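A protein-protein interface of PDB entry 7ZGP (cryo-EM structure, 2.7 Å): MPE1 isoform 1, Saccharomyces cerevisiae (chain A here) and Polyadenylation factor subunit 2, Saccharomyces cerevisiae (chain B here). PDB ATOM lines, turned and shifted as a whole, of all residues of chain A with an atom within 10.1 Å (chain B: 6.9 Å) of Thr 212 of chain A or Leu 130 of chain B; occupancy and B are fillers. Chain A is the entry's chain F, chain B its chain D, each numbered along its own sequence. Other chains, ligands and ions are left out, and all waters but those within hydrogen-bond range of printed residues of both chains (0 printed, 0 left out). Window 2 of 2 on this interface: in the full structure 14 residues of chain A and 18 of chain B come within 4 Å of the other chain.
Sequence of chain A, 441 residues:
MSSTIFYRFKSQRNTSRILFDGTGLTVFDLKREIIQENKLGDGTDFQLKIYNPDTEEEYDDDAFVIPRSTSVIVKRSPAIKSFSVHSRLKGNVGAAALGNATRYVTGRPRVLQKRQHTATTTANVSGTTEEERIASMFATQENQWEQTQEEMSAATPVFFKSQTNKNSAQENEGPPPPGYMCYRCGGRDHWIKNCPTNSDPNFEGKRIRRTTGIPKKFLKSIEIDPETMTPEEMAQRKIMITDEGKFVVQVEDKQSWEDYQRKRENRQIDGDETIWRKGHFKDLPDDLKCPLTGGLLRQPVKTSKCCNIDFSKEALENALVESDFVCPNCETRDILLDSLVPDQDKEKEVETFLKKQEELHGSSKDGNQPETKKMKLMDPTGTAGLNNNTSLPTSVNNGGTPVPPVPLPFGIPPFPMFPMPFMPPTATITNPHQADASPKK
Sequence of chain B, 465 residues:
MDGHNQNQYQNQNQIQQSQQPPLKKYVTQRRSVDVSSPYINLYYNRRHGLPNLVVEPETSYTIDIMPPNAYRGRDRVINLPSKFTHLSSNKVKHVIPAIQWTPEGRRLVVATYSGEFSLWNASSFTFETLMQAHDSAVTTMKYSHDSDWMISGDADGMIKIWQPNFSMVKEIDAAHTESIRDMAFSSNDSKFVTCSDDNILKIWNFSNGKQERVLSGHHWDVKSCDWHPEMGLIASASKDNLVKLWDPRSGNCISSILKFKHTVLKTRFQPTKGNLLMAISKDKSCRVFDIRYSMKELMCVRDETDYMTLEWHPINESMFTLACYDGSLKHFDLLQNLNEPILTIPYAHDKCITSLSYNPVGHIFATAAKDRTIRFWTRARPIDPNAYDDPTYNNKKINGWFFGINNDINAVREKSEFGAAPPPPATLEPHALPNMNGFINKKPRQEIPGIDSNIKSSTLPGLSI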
ATOM      1  N   ILE A 208     -37.796   3.914  23.320  1.00  0.00           N
ATOM      2  CA  ILE A 208     -37.935   3.604  21.903  1.00  0.00           C
ATOM      3  C   ILE A 208     -36.951   4.466  21.125  1.00  0.00           C
ATOM      4  O   ILE A 208     -36.900   5.687  21.312  1.00  0.00           O
ATOM      5  CB  ILE A 208     -39.382   3.810  21.413  1.00  0.00           C
ATOM      6  CG1 ILE A 208     -39.479   3.574  19.905  1.00  0.00           C
ATOM      7  CG2 ILE A 208     -39.908   5.188  21.806  1.00  0.00           C
ATOM      8  CD1 ILE A 208     -40.899   3.443  19.406  1.00  0.00           C
ATOM      9  N   ARG A 209     -36.164   3.829  20.265  1.00  0.00           N
ATOM     10  CA  ARG A 209     -35.079   4.495  19.566  1.00  0.00           C
ATOM     11  C   ARG A 209     -35.557   5.085  18.241  1.00  0.00           C
ATOM     12  O   ARG A 209     -36.662   4.815  17.766  1.00  0.00           O
ATOM     13  CB  ARG A 209     -33.926   3.522  19.326  1.00  0.00           C
ATOM     14  CG  ARG A 209     -33.597   2.649  20.524  1.00  0.00           C
ATOM     15  CD  ARG A 209     -32.721   3.391  21.515  1.00  0.00           C
ATOM     16  NE  ARG A 209     -32.450   2.597  22.707  1.00  0.00           N
ATOM     17  CZ  ARG A 209     -32.593   3.040  23.948  1.00  0.00           C
ATOM     18  NH1 ARG A 209     -33.013   4.269  24.199  1.00  0.00           N
ATOM     19  NH2 ARG A 209     -32.307   2.229  24.962  1.00  0.00           N
ATOM     20  N   ARG A 210     -34.697   5.904  17.643  1.00  0.00           N
ATOM     21  CA  ARG A 210     -34.948   6.532  16.355  1.00  0.00           C
ATOM     22  C   ARG A 210     -33.826   6.174  15.393  1.00  0.00           C
ATOM     23  O   ARG A 210     -32.667   6.047  15.798  1.00  0.00           O
ATOM     24  CB  ARG A 210     -35.053   8.054  16.493  1.00  0.00           C
ATOM     25  CG  ARG A 210     -35.593   8.759  15.263  1.00  0.00           C
ATOM     26  CD  ARG A 210     -36.192  10.110  15.617  1.00  0.00           C
ATOM     27  NE  ARG A 210     -35.188  11.038  16.122  1.00  0.00           N
ATOM     28  CZ  ARG A 210     -34.323  11.696  15.361  1.00  0.00           C
ATOM     29  NH1 ARG A 210     -34.306  11.547  14.046  1.00  0.00           N
ATOM     30  NH2 ARG A 210     -33.453  12.522  15.934  1.00  0.00           N
ATOM     31  N   THR A 211     -34.170   6.018  14.114  1.00  0.00           N
ATOM     32  CA  THR A 211     -33.179   5.675  13.100  1.00  0.00           C
ATOM     33  C   THR A 211     -32.319   6.887  12.772  1.00  0.00           C
ATOM     34  O   THR A 211     -32.622   7.633  11.837  1.00  0.00           O
ATOM     35  CB  THR A 211     -33.859   5.160  11.831  1.00  0.00           C
ATOM     36  OG1 THR A 211     -34.293   6.270  11.038  1.00  0.00           O
ATOM     37  CG2 THR A 211     -35.063   4.313  12.185  1.00  0.00           C
ATOM     38  N   THR A 212     -31.243   7.093  13.531  1.00  0.00           N
ATOM     39  CA  THR A 212     -30.454   8.315  13.377  1.00  0.00           C
ATOM     40  C   THR A 212     -29.494   8.214  12.196  1.00  0.00           C
ATOM     41  O   THR A 212     -29.615   8.955  11.216  1.00  0.00           O
ATOM     42  CB  THR A 212     -29.693   8.612  14.673  1.00  0.00           C
ATOM     43  OG1 THR A 212     -30.487   8.211  15.797  1.00  0.00           O
ATOM     44  CG2 THR A 212     -29.387  10.094  14.782  1.00  0.00           C
ATOM     45  N   GLY A 213     -28.545   7.290  12.265  1.00  0.00           N
ATOM     46  CA  GLY A 213     -27.549   7.152  11.226  1.00  0.00           C
ATOM     47  C   GLY A 213     -27.846   6.124  10.164  1.00  0.00           C
ATOM     48  O   GLY A 213     -27.020   5.913   9.272  1.00  0.00           O
ATOM     49  N   ILE A 214     -28.999   5.476  10.227  1.00  0.00           N
ATOM     50  CA  ILE A 214     -29.290   4.355   9.333  1.00  0.00           C
ATOM     51  C   ILE A 214     -29.844   4.907   8.023  1.00  0.00           C
ATOM     52  O   ILE A 214     -30.850   5.632   8.043  1.00  0.00           O
ATOM     53  CB  ILE A 214     -30.277   3.404   9.992  1.00  0.00           C
ATOM     54  CG1 ILE A 214     -29.768   3.033  11.386  1.00  0.00           C
ATOM     55  CG2 ILE A 214     -30.398   2.145   9.163  1.00  0.00           C
ATOM     56  CD1 ILE A 214     -30.654   2.069  12.131  1.00  0.00           C
ATOM     57  N   PRO A 215     -29.232   4.597   6.877  1.00  0.00           N
ATOM     58  CA  PRO A 215     -29.613   5.285   5.634  1.00  0.00           C
ATOM     59  C   PRO A 215     -30.827   4.703   4.925  1.00  0.00           C
ATOM     60  O   PRO A 215     -30.806   4.540   3.701  1.00  0.00           O
ATOM     61  CB  PRO A 215     -28.359   5.144   4.758  1.00  0.00           C
ATOM     62  CG  PRO A 215     -27.303   4.509   5.626  1.00  0.00           C
ATOM     63  CD  PRO A 215     -28.019   3.787   6.709  1.00  0.00           C
ATOM     64  N   LYS A 216     -31.878   4.364   5.673  1.00  0.00           N
ATOM     65  CA  LYS A 216     -33.231   4.199   5.143  1.00  0.00           C
ATOM     66  C   LYS A 216     -33.356   3.033   4.160  1.00  0.00           C
ATOM     67  O   LYS A 216     -34.469   2.605   3.834  1.00  0.00           O
ATOM     68  CB  LYS A 216     -33.680   5.527   4.509  1.00  0.00           C
ATOM     69  CG  LYS A 216     -34.604   5.446   3.302  1.00  0.00           C
ATOM     70  CD  LYS A 216     -35.641   6.556   3.330  1.00  0.00           C
ATOM     71  CE  LYS A 216     -36.469   6.561   2.057  1.00  0.00           C
ATOM     72  NZ  LYS A 216     -36.797   5.180   1.608  1.00  0.00           N
ATOM     73  N   LEU A 219     -33.481  -0.386   6.494  1.00  0.00           N
ATOM     74  CA  LEU A 219     -34.670  -0.394   7.333  1.00  0.00           C
ATOM     75  C   LEU A 219     -35.845  -0.934   6.532  1.00  0.00           C
ATOM     76  O   LEU A 219     -36.145  -0.428   5.445  1.00  0.00           O
ATOM     77  CB  LEU A 219     -35.000   1.011   7.843  1.00  0.00           C
ATOM     78  CG  LEU A 219     -33.931   1.778   8.617  1.00  0.00           C
ATOM     79  CD1 LEU A 219     -34.285   3.251   8.675  1.00  0.00           C
ATOM     80  CD2 LEU A 219     -33.790   1.206  10.016  1.00  0.00           C
ATOM     81  N   ILE A 241     -38.096   0.656  17.273  1.00  0.00           N
ATOM     82  CA  ILE A 241     -37.360   1.735  16.619  1.00  0.00           C
ATOM     83  C   ILE A 241     -38.213   2.260  15.472  1.00  0.00           C
ATOM     84  O   ILE A 241     -38.759   1.486  14.682  1.00  0.00           O
ATOM     85  CB  ILE A 241     -35.964   1.262  16.143  1.00  0.00           C
ATOM     86  CG1 ILE A 241     -35.312   2.298  15.230  1.00  0.00           C
ATOM     87  CG2 ILE A 241     -36.058  -0.069  15.432  1.00  0.00           C
ATOM     88  CD1 ILE A 241     -33.966   1.857  14.694  1.00  0.00           C
ATOM     89  N   THR A 242     -38.332   3.584  15.392  1.00  0.00           N
ATOM     90  CA  THR A 242     -39.122   4.233  14.355  1.00  0.00           C
ATOM     91  C   THR A 242     -38.412   5.505  13.925  1.00  0.00           C
ATOM     92  O   THR A 242     -37.704   6.132  14.715  1.00  0.00           O
ATOM     93  CB  THR A 242     -40.537   4.565  14.842  1.00  0.00           C
ATOM     94  OG1 THR A 242     -41.152   5.486  13.934  1.00  0.00           O
ATOM     95  CG2 THR A 242     -40.485   5.196  16.223  1.00  0.00           C
ATOM     96  N   ASP A 243     -38.601   5.887  12.661  1.00  0.00           N
ATOM     97  CA  ASP A 243     -37.982   7.104  12.143  1.00  0.00           C
ATOM     98  C   ASP A 243     -38.955   8.278  12.086  1.00  0.00           C
ATOM     99  O   ASP A 243     -38.806   9.244  12.842  1.00  0.00           O
ATOM    100  CB  ASP A 243     -37.402   6.826  10.750  1.00  0.00           C
ATOM    101  CG  ASP A 243     -38.337   5.998   9.886  1.00  0.00           C
ATOM    102  OD1 ASP A 243     -39.421   5.624  10.380  1.00  0.00           O
ATOM    103  OD2 ASP A 243     -37.997   5.735   8.713  1.00  0.00           O
ATOM    104  N   GLU A 244     -39.984   8.187  11.242  1.00  0.00           N
ATOM    105  CA  GLU A 244     -41.027   9.212  11.123  1.00  0.00           C
ATOM    106  C   GLU A 244     -42.357   8.460  11.050  1.00  0.00           C
ATOM    107  O   GLU A 244     -42.819   8.101   9.964  1.00  0.00           O
ATOM    108  CB  GLU A 244     -40.860  10.119   9.905  1.00  0.00           C
ATOM    109  CG  GLU A 244     -39.871  11.312   9.943  1.00  0.00           C
ATOM    110  CD  GLU A 244     -38.570  11.074  10.677  1.00  0.00           C
ATOM    111  OE1 GLU A 244     -38.263  11.849  11.610  1.00  0.00           O
ATOM    112  OE2 GLU A 244     -37.819  10.159  10.279  1.00  0.00           O
ATOM    113  N   VAL A 248     -39.876   0.676  11.843  1.00  0.00           N
ATOM    114  CA  VAL A 248     -38.966  -0.065  10.981  1.00  0.00           C
ATOM    115  C   VAL A 248     -38.022  -0.876  11.861  1.00  0.00           C
ATOM    116  O   VAL A 248     -38.096  -0.841  13.090  1.00  0.00           O
ATOM    117  CB  VAL A 248     -38.167   0.860  10.038  1.00  0.00           C
ATOM    118  CG1 VAL A 248     -39.091   1.552   9.048  1.00  0.00           C
ATOM    119  CG2 VAL A 248     -37.388   1.879  10.842  1.00  0.00           C
ATOM    120  N   GLN A 250     -33.689  -2.398  11.663  1.00  0.00           N
ATOM    121  CA  GLN A 250     -32.434  -2.451  10.926  1.00  0.00           C
ATOM    122  C   GLN A 250     -32.139  -3.875  10.483  1.00  0.00           C
ATOM    123  O   GLN A 250     -32.323  -4.828  11.247  1.00  0.00           O
ATOM    124  CB  GLN A 250     -31.279  -1.918  11.771  1.00  0.00           C
ATOM    125  CG  GLN A 250     -30.239  -1.166  10.956  1.00  0.00           C
ATOM    126  CD  GLN A 250     -28.836  -1.320  11.505  1.00  0.00           C
ATOM    127  OE1 GLN A 250     -28.647  -1.751  12.643  1.00  0.00           O
ATOM    128  NE2 GLN A 250     -27.842  -0.967  10.699  1.00  0.00           N
ATOM    129  N   ASN B  90     -22.044  14.913  24.404  1.00  0.00           N
ATOM    130  CA  ASN B  90     -23.106  14.799  23.418  1.00  0.00           C
ATOM    131  C   ASN B  90     -24.206  15.819  23.702  1.00  0.00           C
ATOM    132  O   ASN B  90     -24.288  16.399  24.789  1.00  0.00           O
ATOM    133  CB  ASN B  90     -23.686  13.386  23.417  1.00  0.00           C
ATOM    134  CG  ASN B  90     -22.729  12.363  22.839  1.00  0.00           C
ATOM    135  OD1 ASN B  90     -22.471  12.348  21.636  1.00  0.00           O
ATOM    136  ND2 ASN B  90     -22.197  11.500  23.697  1.00  0.00           N
ATOM    137  N   LYS B  91     -25.058  16.040  22.697  1.00  0.00           N
ATOM    138  CA  LYS B  91     -26.204  16.923  22.890  1.00  0.00           C
ATOM    139  C   LYS B  91     -27.129  16.388  23.974  1.00  0.00           C
ATOM    140  O   LYS B  91     -27.606  17.147  24.826  1.00  0.00           O
ATOM    141  CB  LYS B  91     -26.966  17.094  21.575  1.00  0.00           C
ATOM    142  CG  LYS B  91     -26.292  18.016  20.577  1.00  0.00           C
ATOM    143  CD  LYS B  91     -27.156  18.203  19.340  1.00  0.00           C
ATOM    144  CE  LYS B  91     -26.486  19.120  18.331  1.00  0.00           C
ATOM    145  NZ  LYS B  91     -27.317  19.295  17.109  1.00  0.00           N
ATOM    146  N   VAL B  92     -27.390  15.085  23.962  1.00  0.00           N
ATOM    147  CA  VAL B  92     -28.161  14.422  25.004  1.00  0.00           C
ATOM    148  C   VAL B  92     -27.177  13.748  25.948  1.00  0.00           C
ATOM    149  O   VAL B  92     -26.395  12.886  25.532  1.00  0.00           O
ATOM    150  CB  VAL B  92     -29.151  13.406  24.415  1.00  0.00           C
ATOM    151  CG1 VAL B  92     -30.086  12.892  25.497  1.00  0.00           C
ATOM    152  CG2 VAL B  92     -29.941  14.037  23.281  1.00  0.00           C
ATOM    153  N   HIS B  94     -25.948  11.228  27.880  1.00  0.00           N
ATOM    154  CA  HIS B  94     -26.196   9.806  28.044  1.00  0.00           C
ATOM    155  C   HIS B  94     -25.002   9.147  28.715  1.00  0.00           C
ATOM    156  O   HIS B  94     -23.860   9.584  28.554  1.00  0.00           O
ATOM    157  CB  HIS B  94     -26.468   9.129  26.696  1.00  0.00           C
ATOM    158  CG  HIS B  94     -27.908   9.145  26.291  1.00  0.00           C
ATOM    159  ND1 HIS B  94     -28.907   8.610  27.075  1.00  0.00           N
ATOM    160  CD2 HIS B  94     -28.519   9.632  25.186  1.00  0.00           C
ATOM    161  CE1 HIS B  94     -30.070   8.767  26.470  1.00  0.00           C
ATOM    162  NE2 HIS B  94     -29.863   9.385  25.322  1.00  0.00           N
ATOM    163  N   VAL B 110     -17.697   6.740  20.477  1.00  0.00           N
ATOM    164  CA  VAL B 110     -18.267   6.874  21.812  1.00  0.00           C
ATOM    165  C   VAL B 110     -19.625   6.189  21.800  1.00  0.00           C
ATOM    166  O   VAL B 110     -20.596   6.720  21.249  1.00  0.00           O
ATOM    167  CB  VAL B 110     -18.387   8.343  22.237  1.00  0.00           C
ATOM    168  CG1 VAL B 110     -19.119   8.457  23.561  1.00  0.00           C
ATOM    169  CG2 VAL B 110     -17.013   8.980  22.325  1.00  0.00           C
ATOM    170  N   THR B 112     -23.043   5.016  23.535  1.00  0.00           N
ATOM    171  CA  THR B 112     -23.911   5.573  24.559  1.00  0.00           C
ATOM    172  C   THR B 112     -24.833   4.498  25.115  1.00  0.00           C
ATOM    173  O   THR B 112     -25.000   3.423  24.533  1.00  0.00           O
ATOM    174  CB  THR B 112     -24.741   6.737  24.009  1.00  0.00           C
ATOM    175  OG1 THR B 112     -25.843   6.225  23.252  1.00  0.00           O
ATOM    176  CG2 THR B 112     -23.889   7.624  23.119  1.00  0.00           C
ATOM    177  N   SER B 114     -27.920   4.645  25.146  1.00  0.00           N
ATOM    178  CA  SER B 114     -29.061   4.548  24.248  1.00  0.00           C
ATOM    179  C   SER B 114     -28.750   3.752  22.987  1.00  0.00           C
ATOM    180  O   SER B 114     -29.519   3.818  22.023  1.00  0.00           O
ATOM    181  CB  SER B 114     -29.553   5.946  23.868  1.00  0.00           C
ATOM    182  OG  SER B 114     -28.541   6.677  23.197  1.00  0.00           O
ATOM    183  N   GLU B 116     -26.175   4.105  20.741  1.00  0.00           N
ATOM    184  CA  GLU B 116     -25.803   4.975  19.638  1.00  0.00           C
ATOM    185  C   GLU B 116     -24.289   5.050  19.521  1.00  0.00           C
ATOM    186  O   GLU B 116     -23.563   4.854  20.500  1.00  0.00           O
ATOM    187  CB  GLU B 116     -26.380   6.381  19.830  1.00  0.00           C
ATOM    188  CG  GLU B 116     -27.885   6.446  19.667  1.00  0.00           C
ATOM    189  CD  GLU B 116     -28.465   7.778  20.095  1.00  0.00           C
ATOM    190  OE1 GLU B 116     -28.060   8.290  21.160  1.00  0.00           O
ATOM    191  OE2 GLU B 116     -29.329   8.312  19.369  1.00  0.00           O
ATOM    192  N   PHE B 117     -23.818   5.331  18.310  1.00  0.00           N
ATOM    193  CA  PHE B 117     -22.404   5.569  18.047  1.00  0.00           C
ATOM    194  C   PHE B 117     -22.220   7.039  17.708  1.00  0.00           C
ATOM    195  O   PHE B 117     -22.844   7.547  16.771  1.00  0.00           O
ATOM    196  CB  PHE B 117     -21.892   4.694  16.902  1.00  0.00           C
ATOM    197  CG  PHE B 117     -21.601   3.277  17.297  1.00  0.00           C
ATOM    198  CD1 PHE B 117     -21.618   2.893  18.626  1.00  0.00           C
ATOM    199  CD2 PHE B 117     -21.293   2.329  16.336  1.00  0.00           C
ATOM    200  CE1 PHE B 117     -21.347   1.590  18.987  1.00  0.00           C
ATOM    201  CE2 PHE B 117     -21.019   1.024  16.692  1.00  0.00           C
ATOM    202  CZ  PHE B 117     -21.047   0.654  18.019  1.00  0.00           C
ATOM    203  N   SER B 118     -21.371   7.719  18.471  1.00  0.00           N
ATOM    204  CA  SER B 118     -20.980   9.092  18.185  1.00  0.00           C
ATOM    205  C   SER B 118     -19.493   9.107  17.878  1.00  0.00           C
ATOM    206  O   SER B 118     -18.683   8.655  18.694  1.00  0.00           O
ATOM    207  CB  SER B 118     -21.303  10.022  19.356  1.00  0.00           C
ATOM    208  OG  SER B 118     -20.809   9.500  20.574  1.00  0.00           O
ATOM    209  N   LEU B 119     -19.139   9.615  16.706  1.00  0.00           N
ATOM    210  CA  LEU B 119     -17.747   9.730  16.309  1.00  0.00           C
ATOM    211  C   LEU B 119     -17.202  11.091  16.714  1.00  0.00           C
ATOM    212  O   LEU B 119     -17.947  12.066  16.837  1.00  0.00           O
ATOM    213  CB  LEU B 119     -17.597   9.523  14.804  1.00  0.00           C
ATOM    214  CG  LEU B 119     -18.109   8.174  14.302  1.00  0.00           C
ATOM    215  CD1 LEU B 119     -17.776   7.985  12.839  1.00  0.00           C
ATOM    216  CD2 LEU B 119     -17.527   7.048  15.134  1.00  0.00           C
ATOM    217  N   PHE B 127     -17.202  16.538  16.515  1.00  0.00           N
ATOM    218  CA  PHE B 127     -18.214  15.899  15.681  1.00  0.00           C
ATOM    219  C   PHE B 127     -19.465  15.693  16.521  1.00  0.00           C
ATOM    220  O   PHE B 127     -19.392  15.627  17.751  1.00  0.00           O
ATOM    221  CB  PHE B 127     -17.734  14.560  15.108  1.00  0.00           C
ATOM    222  CG  PHE B 127     -18.598  14.033  14.001  1.00  0.00           C
ATOM    223  CD1 PHE B 127     -18.649  14.681  12.781  1.00  0.00           C
ATOM    224  CD2 PHE B 127     -19.366  12.897  14.182  1.00  0.00           C
ATOM    225  CE1 PHE B 127     -19.443  14.203  11.761  1.00  0.00           C
ATOM    226  CE2 PHE B 127     -20.162  12.414  13.166  1.00  0.00           C
ATOM    227  CZ  PHE B 127     -20.199  13.068  11.954  1.00  0.00           C
ATOM    228  N   GLU B 128     -20.613  15.594  15.847  1.00  0.00           N
ATOM    229  CA  GLU B 128     -21.883  15.442  16.554  1.00  0.00           C
ATOM    230  C   GLU B 128     -22.818  14.379  15.992  1.00  0.00           C
ATOM    231  O   GLU B 128     -23.648  13.871  16.753  1.00  0.00           O
ATOM    232  CB  GLU B 128     -22.634  16.778  16.595  1.00  0.00           C
ATOM    233  CG  GLU B 128     -22.393  17.581  17.862  1.00  0.00           C
ATOM    234  CD  GLU B 128     -23.109  16.994  19.061  1.00  0.00           C
ATOM    235  OE1 GLU B 128     -24.138  16.313  18.865  1.00  0.00           O
ATOM    236  OE2 GLU B 128     -22.642  17.212  20.198  1.00  0.00           O
ATOM    237  N   THR B 129     -22.733  14.018  14.713  1.00  0.00           N
ATOM    238  CA  THR B 129     -23.764  13.189  14.100  1.00  0.00           C
ATOM    239  C   THR B 129     -23.730  11.767  14.657  1.00  0.00           C
ATOM    240  O   THR B 129     -22.674  11.130  14.711  1.00  0.00           O
ATOM    241  CB  THR B 129     -23.598  13.171  12.581  1.00  0.00           C
ATOM    242  OG1 THR B 129     -23.710  14.506  12.073  1.00  0.00           O
ATOM    243  CG2 THR B 129     -24.666  12.302  11.936  1.00  0.00           C
ATOM    244  N   LEU B 130     -24.901  11.275  15.059  1.00  0.00           N
ATOM    245  CA  LEU B 130     -25.058   9.994  15.726  1.00  0.00           C
ATOM    246  C   LEU B 130     -25.259   8.875  14.706  1.00  0.00           C
ATOM    247  O   LEU B 130     -25.308   9.102  13.495  1.00  0.00           O
ATOM    248  CB  LEU B 130     -26.230  10.067  16.702  1.00  0.00           C
ATOM    249  CG  LEU B 130     -25.955  10.759  18.035  1.00  0.00           C
ATOM    250  CD1 LEU B 130     -27.176  10.698  18.926  1.00  0.00           C
ATOM    251  CD2 LEU B 130     -24.779  10.099  18.716  1.00  0.00           C
ATOM    252  N   MET B 131     -25.379   7.643  15.201  1.00  0.00           N
ATOM    253  CA  MET B 131     -25.546   6.482  14.336  1.00  0.00           C
ATOM    254  C   MET B 131     -26.658   5.527  14.745  1.00  0.00           C
ATOM    255  O   MET B 131     -27.206   4.854  13.863  1.00  0.00           O
ATOM    256  CB  MET B 131     -24.235   5.687  14.252  1.00  0.00           C
ATOM    257  CG  MET B 131     -23.946   5.123  12.878  1.00  0.00           C
ATOM    258  SD  MET B 131     -22.186   5.150  12.513  1.00  0.00           S
ATOM    259  CE  MET B 131     -21.928   6.904  12.263  1.00  0.00           C
ATOM    260  N   GLN B 132     -27.008   5.438  16.029  1.00  0.00           N
ATOM    261  CA  GLN B 132     -27.995   4.476  16.525  1.00  0.00           C
ATOM    262  C   GLN B 132     -27.588   3.047  16.149  1.00  0.00           C
ATOM    263  O   GLN B 132     -28.234   2.362  15.355  1.00  0.00           O
ATOM    264  CB  GLN B 132     -29.404   4.805  16.017  1.00  0.00           C
ATOM    265  CG  GLN B 132     -30.499   4.021  16.719  1.00  0.00           C
ATOM    266  CD  GLN B 132     -30.481   4.213  18.221  1.00  0.00           C
ATOM    267  OE1 GLN B 132     -30.732   5.309  18.721  1.00  0.00           O
ATOM    268  NE2 GLN B 132     -30.179   3.146  18.950  1.00  0.00           N
ATOM    269  N   ALA B 133     -26.466   2.630  16.733  1.00  0.00           N
ATOM    270  CA  ALA B 133     -25.895   1.326  16.414  1.00  0.00           C
ATOM    271  C   ALA B 133     -26.820   0.194  16.846  1.00  0.00           C
ATOM    272  O   ALA B 133     -27.274  -0.607  16.021  1.00  0.00           O
ATOM    273  CB  ALA B 133     -24.526   1.184  17.076  1.00  0.00           C
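The side-chain hydroxyl (OG) of Ser 114 of chain B sits at hydrogen-bond distance from the side-chain hydroxyl (OG1) of Thr 112 of chain B (2.7 Å).
OG of Ser 114 of chain B lies within hydrogen-bond range of OE1 of Glu 116 of chain B (2.6 Å).
O of Ser 114 of chain B is in hydrogen-bond range of NE2 of Gln 132 of chain B (3.2 Å).
The backbone carbonyl oxygen (O) of Phe 117 of chain B is in hydrogen-bond range of the backbone NH (N) of Met 131 of chain B.
N of Thr 242 of chain A lies within hydrogen-bond range of O of Arg 209 of chain A, 3.2 Å away.
OG1 of Thr 212 of chain A sits at hydrogen-bond distance from O of Arg 210 of chain A.
O of Ser 114 of chain B lies within hydrogen-bond range of NE of Arg 209 of chain A (3.2 Å).
N of Gly 213 of chain A sits at hydrogen-bond distance from O of Met 131 of chain B, at 3.2 Å.
Hydrophobic or aromatic side chains of chain B within 4 Å of the printed part of chain A: Leu 130.
Of the 16 printed residues of chain A, 5 touch a printed residue of chain B.
Printed residues of chain A that touch a printed residue of chain B: Arg 209, Arg 210, Thr 212, Gly 213 and Gln 250.
Of chain B, only Glu 116 (3.8 Å), Leu 130 (3.7 Å) and Gln 132 (3.6 Å) come within 4 Å of Thr 212 of chain A.
Of chain A, only Thr 212 and Gly 213 come within 4 Å of Leu 130 of chain B.
No residue of chain A comes within 4 Å of Thr 129 of chain B.
Of chain A, only Arg 209, Arg 210 and Thr 212 come within 4 Å of Gln 132 of chain B.
Of the printed residues of chain A, Ser 114 of chain B touches Arg 209 (3.2 Å).
Printed residues of chain A within 4 Å of Glu 116 of chain B: Thr 212 (3.8 Å).
Printed residues of chain B within 4 Å of Gln 250 of chain A: Ala 133 (3.8 Å).
Printed residues of chain B within 4 Å of Arg 209 of chain A: Ser 114 and Gln 132.
Ile 241 of chain A touches none of the printed residues of chain B.
The nearest residue of chain A that does not touch Leu 130 of chain B is Ile 214 of chain A (6.1 Å).
The nearest printed residue of chain A that does not touch Ala 133 of chain B is Ile 214 of chain A (5.8 Å).
CD of Arg 209 of chain A touches NE2 of Gln 132 of chain B (3.6 Å).
Gln 132 of chain B touches Arg 210 of chain A.
OE2 of Glu 116 of chain B touches OG1 of Thr 212 of chain A, 3.8 Å away.
CB of Leu 130 of chain B touches CG2 of Thr 212 of chain A, 3.7 Å away.
Thr 212 of chain A touches Gln 132 of chain B (OG1 to CB, 3.6 Å).
CA of Gly 213 of chain A touches O of Leu 130 of chain B, at 3.7 Å.
OE1 of Gln 250 of chain A touches O of Ala 133 of chain B (3.8 Å).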
